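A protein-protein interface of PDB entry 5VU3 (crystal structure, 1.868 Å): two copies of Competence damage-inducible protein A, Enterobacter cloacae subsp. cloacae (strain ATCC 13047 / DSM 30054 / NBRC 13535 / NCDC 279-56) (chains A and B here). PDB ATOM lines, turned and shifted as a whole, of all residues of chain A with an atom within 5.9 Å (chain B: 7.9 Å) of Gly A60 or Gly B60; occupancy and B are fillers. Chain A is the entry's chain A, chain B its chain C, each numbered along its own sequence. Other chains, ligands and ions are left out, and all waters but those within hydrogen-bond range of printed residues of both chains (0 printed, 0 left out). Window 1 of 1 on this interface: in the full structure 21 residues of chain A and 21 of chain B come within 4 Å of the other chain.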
ATOM      1  N   THR A  33      -6.811 -34.187  25.072  1.00  0.00           N
ATOM      2  CA  THR A  33      -6.643 -33.138  24.075  1.00  0.00           C
ATOM      3  C   THR A  33      -7.990 -32.450  23.876  1.00  0.00           C
ATOM      4  O   THR A  33      -9.041 -32.992  24.235  1.00  0.00           O
ATOM      5  CB  THR A  33      -6.102 -33.695  22.750  1.00  0.00           C
ATOM      6  OG1 THR A  33      -5.832 -32.627  21.828  1.00  0.00           O
ATOM      7  CG2 THR A  33      -7.107 -34.636  22.098  1.00  0.00           C
ATOM      8  N   THR A  34      -7.959 -31.238  23.320  1.00  0.00           N
ATOM      9  CA  THR A  34      -9.170 -30.432  23.205  1.00  0.00           C
ATOM     10  C   THR A  34      -9.223 -29.718  21.861  1.00  0.00           C
ATOM     11  O   THR A  34      -8.193 -29.369  21.277  1.00  0.00           O
ATOM     12  CB  THR A  34      -9.275 -29.375  24.316  1.00  0.00           C
ATOM     13  OG1 THR A  34      -8.101 -28.552  24.300  1.00  0.00           O
ATOM     14  CG2 THR A  34      -9.418 -30.034  25.677  1.00  0.00           C
ATOM     15  N   ALA A  35     -10.447 -29.506  21.381  1.00  0.00           N
ATOM     16  CA  ALA A  35     -10.713 -28.687  20.205  1.00  0.00           C
ATOM     17  C   ALA A  35     -11.846 -27.734  20.552  1.00  0.00           C
ATOM     18  O   ALA A  35     -12.948 -28.180  20.887  1.00  0.00           O
ATOM     19  CB  ALA A  35     -11.077 -29.558  18.999  1.00  0.00           C
ATOM     20  N   SER A  44      -8.260 -24.733  27.102  1.00  0.00           N
ATOM     21  CA  SER A  44      -6.841 -25.071  27.159  1.00  0.00           C
ATOM     22  C   SER A  44      -6.138 -24.323  28.286  1.00  0.00           C
ATOM     23  O   SER A  44      -5.288 -24.891  28.984  1.00  0.00           O
ATOM     24  CB  SER A  44      -6.174 -24.768  25.818  1.00  0.00           C
ATOM     25  OG  SER A  44      -4.767 -24.863  25.925  1.00  0.00           O
ATOM     26  N   TYR A  57      -1.905 -33.481  29.652  1.00  0.00           N
ATOM     27  CA  TYR A  57      -2.440 -32.601  28.622  1.00  0.00           C
ATOM     28  C   TYR A  57      -1.308 -32.148  27.716  1.00  0.00           C
ATOM     29  O   TYR A  57      -0.258 -31.709  28.196  1.00  0.00           O
ATOM     30  CB  TYR A  57      -3.165 -31.393  29.237  1.00  0.00           C
ATOM     31  CG  TYR A  57      -3.874 -30.505  28.228  1.00  0.00           C
ATOM     32  CD1 TYR A  57      -3.532 -29.170  28.095  1.00  0.00           C
ATOM     33  CD2 TYR A  57      -4.893 -31.004  27.417  1.00  0.00           C
ATOM     34  CE1 TYR A  57      -4.172 -28.347  27.174  1.00  0.00           C
ATOM     35  CE2 TYR A  57      -5.539 -30.189  26.490  1.00  0.00           C
ATOM     36  CZ  TYR A  57      -5.178 -28.857  26.384  1.00  0.00           C
ATOM     37  OH  TYR A  57      -5.814 -28.034  25.477  1.00  0.00           O
ATOM     38  N   ASP A  58      -1.521 -32.270  26.406  1.00  0.00           N
ATOM     39  CA  ASP A  58      -0.501 -31.918  25.426  1.00  0.00           C
ATOM     40  C   ASP A  58      -1.058 -30.912  24.415  1.00  0.00           C
ATOM     41  O   ASP A  58      -0.611 -29.764  24.404  1.00  0.00           O
ATOM     42  CB  ASP A  58       0.021 -33.182  24.739  1.00  0.00           C
ATOM     43  CG  ASP A  58       1.240 -32.925  23.869  1.00  0.00           C
ATOM     44  OD1 ASP A  58       1.711 -31.772  23.810  1.00  0.00           O
ATOM     45  OD2 ASP A  58       1.737 -33.883  23.240  1.00  0.00           O
ATOM     46  N   VAL A  59      -2.036 -31.300  23.606  1.00  0.00           N
ATOM     47  CA  VAL A  59      -2.431 -30.539  22.426  1.00  0.00           C
ATOM     48  C   VAL A  59      -3.776 -29.876  22.672  1.00  0.00           C
ATOM     49  O   VAL A  59      -4.729 -30.524  23.123  1.00  0.00           O
ATOM     50  CB  VAL A  59      -2.490 -31.436  21.181  1.00  0.00           C
ATOM     51  CG1 VAL A  59      -3.105 -30.674  19.998  1.00  0.00           C
ATOM     52  CG2 VAL A  59      -1.096 -31.965  20.854  1.00  0.00           C
ATOM     53  N   GLY A  60      -3.858 -28.588  22.345  1.00  0.00           N
ATOM     54  CA  GLY A  60      -5.120 -27.873  22.356  1.00  0.00           C
ATOM     55  C   GLY A  60      -5.293 -27.106  21.065  1.00  0.00           C
ATOM     56  O   GLY A  60      -4.373 -26.409  20.619  1.00  0.00           O
ATOM     57  N   LEU A  61      -6.456 -27.232  20.436  1.00  0.00           N
ATOM     58  CA  LEU A  61      -6.717 -26.549  19.181  1.00  0.00           C
ATOM     59  C   LEU A  61      -7.871 -25.576  19.348  1.00  0.00           C
ATOM     60  O   LEU A  61      -8.875 -25.884  19.998  1.00  0.00           O
ATOM     61  CB  LEU A  61      -7.030 -27.545  18.055  1.00  0.00           C
ATOM     62  CG  LEU A  61      -7.379 -26.930  16.697  1.00  0.00           C
ATOM     63  CD1 LEU A  61      -6.168 -26.264  16.034  1.00  0.00           C
ATOM     64  CD2 LEU A  61      -7.993 -27.988  15.773  1.00  0.00           C
ATOM     65  N   VAL A  62      -7.707 -24.392  18.771  1.00  0.00           N
ATOM     66  CA  VAL A  62      -8.752 -23.382  18.698  1.00  0.00           C
ATOM     67  C   VAL A  62      -9.023 -23.143  17.223  1.00  0.00           C
ATOM     68  O   VAL A  62      -8.083 -22.898  16.457  1.00  0.00           O
ATOM     69  CB  VAL A  62      -8.327 -22.079  19.401  1.00  0.00           C
ATOM     70  CG1 VAL A  62      -9.305 -20.970  19.100  1.00  0.00           C
ATOM     71  CG2 VAL A  62      -8.202 -22.312  20.908  1.00  0.00           C
ATOM     72  N   VAL A  63     -10.287 -23.263  16.812  1.00  0.00           N
ATOM     73  CA  VAL A  63     -10.666 -23.104  15.412  1.00  0.00           C
ATOM     74  C   VAL A  63     -12.018 -22.408  15.350  1.00  0.00           C
ATOM     75  O   VAL A  63     -12.970 -22.829  16.016  1.00  0.00           O
ATOM     76  CB  VAL A  63     -10.725 -24.451  14.656  1.00  0.00           C
ATOM     77  CG1 VAL A  63      -9.330 -24.906  14.259  1.00  0.00           C
ATOM     78  CG2 VAL A  63     -11.425 -25.522  15.485  1.00  0.00           C
ATOM     79  N   ILE A  98      -9.306 -34.666  16.553  1.00  0.00           N
ATOM     80  CA  ILE A  98      -8.266 -34.087  17.410  1.00  0.00           C
ATOM     81  C   ILE A  98      -7.649 -35.160  18.298  1.00  0.00           C
ATOM     82  O   ILE A  98      -6.451 -35.113  18.600  1.00  0.00           O
ATOM     83  CB  ILE A  98      -8.810 -32.902  18.234  1.00  0.00           C
ATOM     84  CG1 ILE A  98      -7.662 -32.137  18.910  1.00  0.00           C
ATOM     85  CG2 ILE A  98      -9.824 -33.364  19.285  1.00  0.00           C
ATOM     86  CD1 ILE A  98      -6.655 -31.533  17.942  1.00  0.00           C
ATOM     87  N   LEU B  32      -4.283 -13.987  10.977  1.00  0.00           N
ATOM     88  CA  LEU B  32      -3.280 -14.322  11.970  1.00  0.00           C
ATOM     89  C   LEU B  32      -3.565 -15.697  12.555  1.00  0.00           C
ATOM     90  O   LEU B  32      -4.724 -16.101  12.698  1.00  0.00           O
ATOM     91  CB  LEU B  32      -3.269 -13.265  13.092  1.00  0.00           C
ATOM     92  CG  LEU B  32      -2.519 -13.593  14.379  1.00  0.00           C
ATOM     93  CD1 LEU B  32      -1.036 -13.472  14.075  1.00  0.00           C
ATOM     94  CD2 LEU B  32      -2.914 -12.652  15.512  1.00  0.00           C
ATOM     95  N   THR B  33      -2.497 -16.421  12.890  1.00  0.00           N
ATOM     96  CA  THR B  33      -2.624 -17.675  13.610  1.00  0.00           C
ATOM     97  C   THR B  33      -1.502 -17.725  14.642  1.00  0.00           C
ATOM     98  O   THR B  33      -0.518 -16.987  14.545  1.00  0.00           O
ATOM     99  CB  THR B  33      -2.556 -18.870  12.647  1.00  0.00           C
ATOM    100  OG1 THR B  33      -2.758 -20.092  13.357  1.00  0.00           O
ATOM    101  CG2 THR B  33      -1.167 -18.944  12.028  1.00  0.00           C
ATOM    102  N   THR B  34      -1.654 -18.590  15.644  1.00  0.00           N
ATOM    103  CA  THR B  34      -0.722 -18.636  16.764  1.00  0.00           C
ATOM    104  C   THR B  34      -0.392 -20.078  17.123  1.00  0.00           C
ATOM    105  O   THR B  34      -1.225 -20.977  16.977  1.00  0.00           O
ATOM    106  CB  THR B  34      -1.292 -17.933  18.013  1.00  0.00           C
ATOM    107  OG1 THR B  34      -2.568 -18.505  18.325  1.00  0.00           O
ATOM    108  CG2 THR B  34      -1.456 -16.438  17.772  1.00  0.00           C
ATOM    109  N   ALA B  35       0.835 -20.289  17.608  1.00  0.00           N
ATOM    110  CA  ALA B  35       1.231 -21.571  18.193  1.00  0.00           C
ATOM    111  C   ALA B  35       1.938 -21.290  19.511  1.00  0.00           C
ATOM    112  O   ALA B  35       2.918 -20.540  19.533  1.00  0.00           O
ATOM    113  CB  ALA B  35       2.147 -22.361  17.249  1.00  0.00           C
ATOM    114  N   GLU B  36       1.454 -21.886  20.601  1.00  0.00           N
ATOM    115  CA  GLU B  36       1.910 -21.556  21.950  1.00  0.00           C
ATOM    116  C   GLU B  36       2.475 -22.785  22.649  1.00  0.00           C
ATOM    117  O   GLU B  36       1.771 -23.787  22.826  1.00  0.00           O
ATOM    118  CB  GLU B  36       0.764 -20.997  22.792  1.00  0.00           C
ATOM    119  CG  GLU B  36       0.161 -19.706  22.295  1.00  0.00           C
ATOM    120  CD  GLU B  36      -1.066 -19.348  23.107  1.00  0.00           C
ATOM    121  OE1 GLU B  36      -0.910 -19.114  24.324  1.00  0.00           O
ATOM    122  OE2 GLU B  36      -2.186 -19.348  22.541  1.00  0.00           O
ATOM    123  N   GLY B  40       0.106 -21.544  27.104  1.00  0.00           N
ATOM    124  CA  GLY B  40      -1.059 -22.336  27.455  1.00  0.00           C
ATOM    125  C   GLY B  40      -2.382 -21.874  26.893  1.00  0.00           C
ATOM    126  O   GLY B  40      -3.426 -22.215  27.456  1.00  0.00           O
ATOM    127  N   GLY B  41      -2.378 -21.105  25.802  1.00  0.00           N
ATOM    128  CA  GLY B  41      -3.601 -20.605  25.206  1.00  0.00           C
ATOM    129  C   GLY B  41      -3.973 -19.191  25.607  1.00  0.00           C
ATOM    130  O   GLY B  41      -4.958 -18.660  25.089  1.00  0.00           O
ATOM    131  N   LEU B  43      -2.507 -16.489  24.790  1.00  0.00           N
ATOM    132  CA  LEU B  43      -2.425 -15.625  23.616  1.00  0.00           C
ATOM    133  C   LEU B  43      -3.674 -15.763  22.757  1.00  0.00           C
ATOM    134  O   LEU B  43      -4.249 -14.760  22.324  1.00  0.00           O
ATOM    135  CB  LEU B  43      -1.168 -15.948  22.802  1.00  0.00           C
ATOM    136  CG  LEU B  43      -0.997 -15.226  21.463  1.00  0.00           C
ATOM    137  CD1 LEU B  43      -1.108 -13.713  21.643  1.00  0.00           C
ATOM    138  CD2 LEU B  43       0.338 -15.597  20.830  1.00  0.00           C
ATOM    139  N   SER B  44      -4.125 -16.998  22.524  1.00  0.00           N
ATOM    140  CA  SER B  44      -5.358 -17.208  21.766  1.00  0.00           C
ATOM    141  C   SER B  44      -6.559 -16.577  22.467  1.00  0.00           C
ATOM    142  O   SER B  44      -7.427 -15.972  21.817  1.00  0.00           O
ATOM    143  CB  SER B  44      -5.580 -18.706  21.555  1.00  0.00           C
ATOM    144  OG  SER B  44      -6.911 -18.961  21.146  1.00  0.00           O
ATOM    145  N   LEU B  47      -6.655 -12.871  21.808  1.00  0.00           N
ATOM    146  CA  LEU B  47      -7.070 -12.556  20.445  1.00  0.00           C
ATOM    147  C   LEU B  47      -8.552 -12.841  20.237  1.00  0.00           C
ATOM    148  O   LEU B  47      -9.228 -12.122  19.492  1.00  0.00           O
ATOM    149  CB  LEU B  47      -6.222 -13.347  19.449  1.00  0.00           C
ATOM    150  CG  LEU B  47      -4.751 -12.942  19.393  1.00  0.00           C
ATOM    151  CD1 LEU B  47      -3.948 -14.013  18.682  1.00  0.00           C
ATOM    152  CD2 LEU B  47      -4.563 -11.580  18.723  1.00  0.00           C
ATOM    153  N   CYS B  48      -9.078 -13.888  20.878  1.00  0.00           N
ATOM    154  CA  CYS B  48     -10.501 -14.186  20.762  1.00  0.00           C
ATOM    155  C   CYS B  48     -11.366 -13.285  21.629  1.00  0.00           C
ATOM    156  O   CYS B  48     -12.594 -13.355  21.527  1.00  0.00           O
ATOM    157  CB  CYS B  48     -10.775 -15.652  21.121  1.00  0.00           C
ATOM    158  SG  CYS B  48     -10.079 -16.861  19.960  1.00  0.00           S
ATOM    159  N   TYR B  57      -8.661 -13.646  12.817  1.00  0.00           N
ATOM    160  CA  TYR B  57      -8.051 -14.720  13.594  1.00  0.00           C
ATOM    161  C   TYR B  57      -8.936 -15.950  13.536  1.00  0.00           C
ATOM    162  O   TYR B  57     -10.141 -15.865  13.789  1.00  0.00           O
ATOM    163  CB  TYR B  57      -7.824 -14.303  15.056  1.00  0.00           C
ATOM    164  CG  TYR B  57      -7.101 -15.350  15.897  1.00  0.00           C
ATOM    165  CD1 TYR B  57      -5.786 -15.706  15.622  1.00  0.00           C
ATOM    166  CD2 TYR B  57      -7.735 -15.973  16.968  1.00  0.00           C
ATOM    167  CE1 TYR B  57      -5.125 -16.663  16.384  1.00  0.00           C
ATOM    168  CE2 TYR B  57      -7.078 -16.924  17.741  1.00  0.00           C
ATOM    169  CZ  TYR B  57      -5.776 -17.262  17.444  1.00  0.00           C
ATOM    170  OH  TYR B  57      -5.121 -18.206  18.206  1.00  0.00           O
ATOM    171  N   ASP B  58      -8.330 -17.094  13.222  1.00  0.00           N
ATOM    172  CA  ASP B  58      -9.086 -18.323  13.038  1.00  0.00           C
ATOM    173  C   ASP B  58      -8.532 -19.460  13.890  1.00  0.00           C
ATOM    174  O   ASP B  58      -9.274 -20.082  14.659  1.00  0.00           O
ATOM    175  CB  ASP B  58      -9.089 -18.705  11.548  1.00  0.00           C
ATOM    176  CG  ASP B  58     -10.002 -19.872  11.240  1.00  0.00           C
ATOM    177  OD1 ASP B  58     -10.795 -20.262  12.124  1.00  0.00           O
ATOM    178  OD2 ASP B  58      -9.937 -20.387  10.099  1.00  0.00           O
ATOM    179  N   VAL B  59      -7.240 -19.744  13.774  1.00  0.00           N
ATOM    180  CA  VAL B  59      -6.667 -20.968  14.315  1.00  0.00           C
ATOM    181  C   VAL B  59      -5.632 -20.625  15.374  1.00  0.00           C
ATOM    182  O   VAL B  59      -4.753 -19.784  15.144  1.00  0.00           O
ATOM    183  CB  VAL B  59      -6.035 -21.830  13.211  1.00  0.00           C
ATOM    184  CG1 VAL B  59      -5.306 -23.035  13.825  1.00  0.00           C
ATOM    185  CG2 VAL B  59      -7.108 -22.270  12.239  1.00  0.00           C
ATOM    186  N   GLY B  60      -5.728 -21.296  16.508  1.00  0.00           N
ATOM    187  CA  GLY B  60      -4.671 -21.260  17.506  1.00  0.00           C
ATOM    188  C   GLY B  60      -4.335 -22.683  17.934  1.00  0.00           C
ATOM    189  O   GLY B  60      -5.221 -23.520  18.044  1.00  0.00           O
ATOM    190  N   LEU B  61      -3.052 -22.925  18.156  1.00  0.00           N
ATOM    191  CA  LEU B  61      -2.582 -24.234  18.599  1.00  0.00           C
ATOM    192  C   LEU B  61      -1.801 -24.083  19.898  1.00  0.00           C
ATOM    193  O   LEU B  61      -0.974 -23.175  20.028  1.00  0.00           O
ATOM    194  CB  LEU B  61      -1.711 -24.892  17.520  1.00  0.00           C
ATOM    195  CG  LEU B  61      -1.311 -26.349  17.762  1.00  0.00           C
ATOM    196  CD1 LEU B  61      -2.532 -27.258  17.776  1.00  0.00           C
ATOM    197  CD2 LEU B  61      -0.309 -26.827  16.713  1.00  0.00           C
ATOM    198  N   VAL B  62      -2.096 -24.949  20.863  1.00  0.00           N
ATOM    199  CA  VAL B  62      -1.320 -25.117  22.088  1.00  0.00           C
ATOM    200  C   VAL B  62      -0.680 -26.498  22.031  1.00  0.00           C
ATOM    201  O   VAL B  62      -1.377 -27.492  21.798  1.00  0.00           O
ATOM    202  CB  VAL B  62      -2.213 -24.978  23.332  1.00  0.00           C
ATOM    203  CG1 VAL B  62      -1.452 -25.366  24.588  1.00  0.00           C
ATOM    204  CG2 VAL B  62      -2.789 -23.557  23.426  1.00  0.00           C
ATOM    205  N   VAL B  63       0.638 -26.572  22.243  1.00  0.00           N
ATOM    206  CA  VAL B  63       1.365 -27.838  22.174  1.00  0.00           C
ATOM    207  C   VAL B  63       2.433 -27.856  23.258  1.00  0.00           C
ATOM    208  O   VAL B  63       3.193 -26.895  23.411  1.00  0.00           O
ATOM    209  CB  VAL B  63       2.003 -28.077  20.789  1.00  0.00           C
ATOM    210  CG1 VAL B  63       1.025 -28.787  19.863  1.00  0.00           C
ATOM    211  CG2 VAL B  63       2.476 -26.772  20.170  1.00  0.00           C
ATOM    212  N   PHE B  64       2.496 -28.954  24.015  1.00  0.00           N
ATOM    213  CA  PHE B  64       3.506 -29.089  25.061  1.00  0.00           C
ATOM    214  C   PHE B  64       4.711 -29.920  24.632  1.00  0.00           C
ATOM    215  O   PHE B  64       5.857 -29.536  24.888  1.00  0.00           O
ATOM    216  CB  PHE B  64       2.906 -29.711  26.329  1.00  0.00           C
ATOM    217  CG  PHE B  64       3.941 -30.064  27.368  1.00  0.00           C
ATOM    218  CD1 PHE B  64       4.244 -31.388  27.653  1.00  0.00           C
ATOM    219  CD2 PHE B  64       4.630 -29.068  28.042  1.00  0.00           C
ATOM    220  CE1 PHE B  64       5.206 -31.708  28.604  1.00  0.00           C
ATOM    221  CE2 PHE B  64       5.591 -29.382  28.995  1.00  0.00           C
ATOM    222  CZ  PHE B  64       5.879 -30.704  29.273  1.00  0.00           C
ATOM    223  N   ALA B  68       4.626 -33.735  19.792  1.00  0.00           N
ATOM    224  CA  ALA B  68       3.567 -33.046  19.059  1.00  0.00           C
ATOM    225  C   ALA B  68       4.118 -31.965  18.140  1.00  0.00           C
ATOM    226  O   ALA B  68       3.551 -31.724  17.068  1.00  0.00           O
ATOM    227  CB  ALA B  68       2.551 -32.443  20.029  1.00  0.00           C
ATOM    228  N   ILE B  72       2.892 -32.724  14.418  1.00  0.00           N
ATOM    229  CA  ILE B  72       1.874 -31.763  13.999  1.00  0.00           C
ATOM    230  C   ILE B  72       2.495 -30.602  13.235  1.00  0.00           C
ATOM    231  O   ILE B  72       2.026 -30.235  12.154  1.00  0.00           O
ATOM    232  CB  ILE B  72       1.051 -31.255  15.199  1.00  0.00           C
ATOM    233  CG1 ILE B  72       0.309 -32.401  15.879  1.00  0.00           C
ATOM    234  CG2 ILE B  72       0.047 -30.212  14.723  1.00  0.00           C
ATOM    235  CD1 ILE B  72      -0.410 -31.964  17.142  1.00  0.00           C
ATOM    236  N   ILE B  98       2.503 -23.473  11.501  1.00  0.00           N
ATOM    237  CA  ILE B  98       1.140 -23.120  11.907  1.00  0.00           C
ATOM    238  C   ILE B  98       0.518 -22.204  10.862  1.00  0.00           C
ATOM    239  O   ILE B  98      -0.688 -22.275  10.593  1.00  0.00           O
ATOM    240  CB  ILE B  98       1.117 -22.495  13.323  1.00  0.00           C
ATOM    241  CG1 ILE B  98      -0.326 -22.413  13.855  1.00  0.00           C
ATOM    242  CG2 ILE B  98       1.769 -21.115  13.339  1.00  0.00           C
ATOM    243  CD1 ILE B  98      -1.023 -23.773  14.004  1.00  0.00           C
ATOM    244  N   ALA B 102      -3.015 -23.158   9.176  1.00  0.00           N
ATOM    245  CA  ALA B 102      -4.125 -22.217   9.267  1.00  0.00           C
ATOM    246  C   ALA B 102      -4.433 -21.505   7.958  1.00  0.00           C
ATOM    247  O   ALA B 102      -5.462 -20.825   7.887  1.00  0.00           O
ATOM    248  CB  ALA B 102      -3.837 -21.162  10.330  1.00  0.00           C
ATOM    249  N   ILE B 108       2.379 -16.043  15.018  1.00  0.00           N
ATOM    250  CA  ILE B 108       3.215 -15.898  16.206  1.00  0.00           C
ATOM    251  C   ILE B 108       3.451 -17.293  16.757  1.00  0.00           C
ATOM    252  O   ILE B 108       2.498 -18.064  16.926  1.00  0.00           O
ATOM    253  CB  ILE B 108       2.553 -15.028  17.295  1.00  0.00           C
ATOM    254  CG1 ILE B 108       2.252 -13.623  16.791  1.00  0.00           C
ATOM    255  CG2 ILE B 108       3.448 -14.987  18.562  1.00  0.00           C
ATOM    256  CD1 ILE B 108       1.297 -12.863  17.681  1.00  0.00           C
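Gly A60 touches just these residues of chain B: Gly B60, Leu B61 and Val B62. Of the printed residues of chain B, Val A63 touches Asp B58 and Val B59. Printed residues of chain B within 4 Å of Leu A61: Gly B60. Of the printed residues of chain B, Val A62 touches Ser B44, Asp B58, Val B59 and Gly B60. Printed residues of chain A within 4 Å of Leu B61: Gly A60 (3.5 Å). Of the printed residues of chain B, Asp A58 touches Val B62, Val B63, Phe B64 and Ala B68. Leu B43 touches none of the printed residues of chain A. Thr B34 touches none of the printed residues of chain A. The nearest residue of chain A that does not touch Gly B60 is Val A63 (5.0 Å).
OG1 of Thr A33 sits at hydrogen-bond distance from O of Val A59. N of Thr A34 sits at hydrogen-bond distance from O of Val A59, at 3.3 Å. OG1 of Thr B33 lies within hydrogen-bond range of O of Val B59, 2.7 Å away. N of Leu B61 sits at hydrogen-bond distance from O of Thr B34, 2.9 Å away. The side-chain carboxylate (OE2) of Glu B36 is in hydrogen-bond range of the backbone NH (N) of Ser B44 (3.0 Å). The backbone carbonyl oxygen (O) of Val B59 lies close to the side-chain hydroxyl (OH) of Tyr B57 (3.5 Å).
The backbone carbonyl oxygen (O) of Gly B40 is in hydrogen-bond range of the side-chain hydroxyl (OG) of Ser A44, at 3.3 Å. The side-chain carboxylate (OD1) of Asp A58 sits at hydrogen-bond distance from the backbone NH (N) of Phe B64 (2.9 Å). The backbone carbonyl oxygen of Gly A60 lies within hydrogen-bond range of the backbone NH of Val B62, at 2.7 Å. N of Val A62 is in hydrogen-bond range of O of Gly B60 (2.7 Å).
Ser A44 touches Val B62, and with the chains exchanged Val A62 touches Ser B44. Val A59 touches Val B63, and with the chains exchanged Val A63 touches Val B59. Gly A60 touches Leu B61, and with the chains exchanged Leu A61 touches Gly B60. Gly A60 touches Val B62, and with the chains exchanged Val A62 touches Gly B60.
Ser A44 touches Val B62. CG1 of Val B63 touches CG2 of Val A59, 3.9 Å away. Val A59 touches Ala B68. Val A59 touches Ile B72. Gly A60 touches Gly B60. Gly A60 touches Leu B61 (O to CA, 3.5 Å). Val A62 touches Ser B44 (CG2 to OG, 3.6 Å). O of Val A62 touches O of Asp B58, at 3.5 Å. Val A62 touches Val B59 (O to CA, 3.2 Å). Val A63 touches Asp B58.
Printed residues of chain B that touch a printed residue of chain A: Gly B40, Ser B44, Asp B58, Val B59, Gly B60, Leu B61, Val B62, Val B63, Phe B64, Ala B68 and Ile B72. Hydrophobic or aromatic side chains of chain B that line the printed part of chain A: Val B59, Leu B61, Val B62, Val B63, Phe B64, Ala B68 and Ile B72. Of the 12 printed residues of chain A, 7 touch a printed residue of chain B. Hydrophobic or aromatic side chains of chain A within 4 Å of the printed part of chain B: Val A59, Leu A61, Val A62 and Val A63. Along chain A the printed residues that touch a printed residue of chain B span positions 44 to 63. Among the printed residues, 20 pairs touch across the chains. Among the printed residues, no Asp or Glu carboxylate lies within 4 Å of a Lys or Arg side-chain nitrogen of the other chain.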
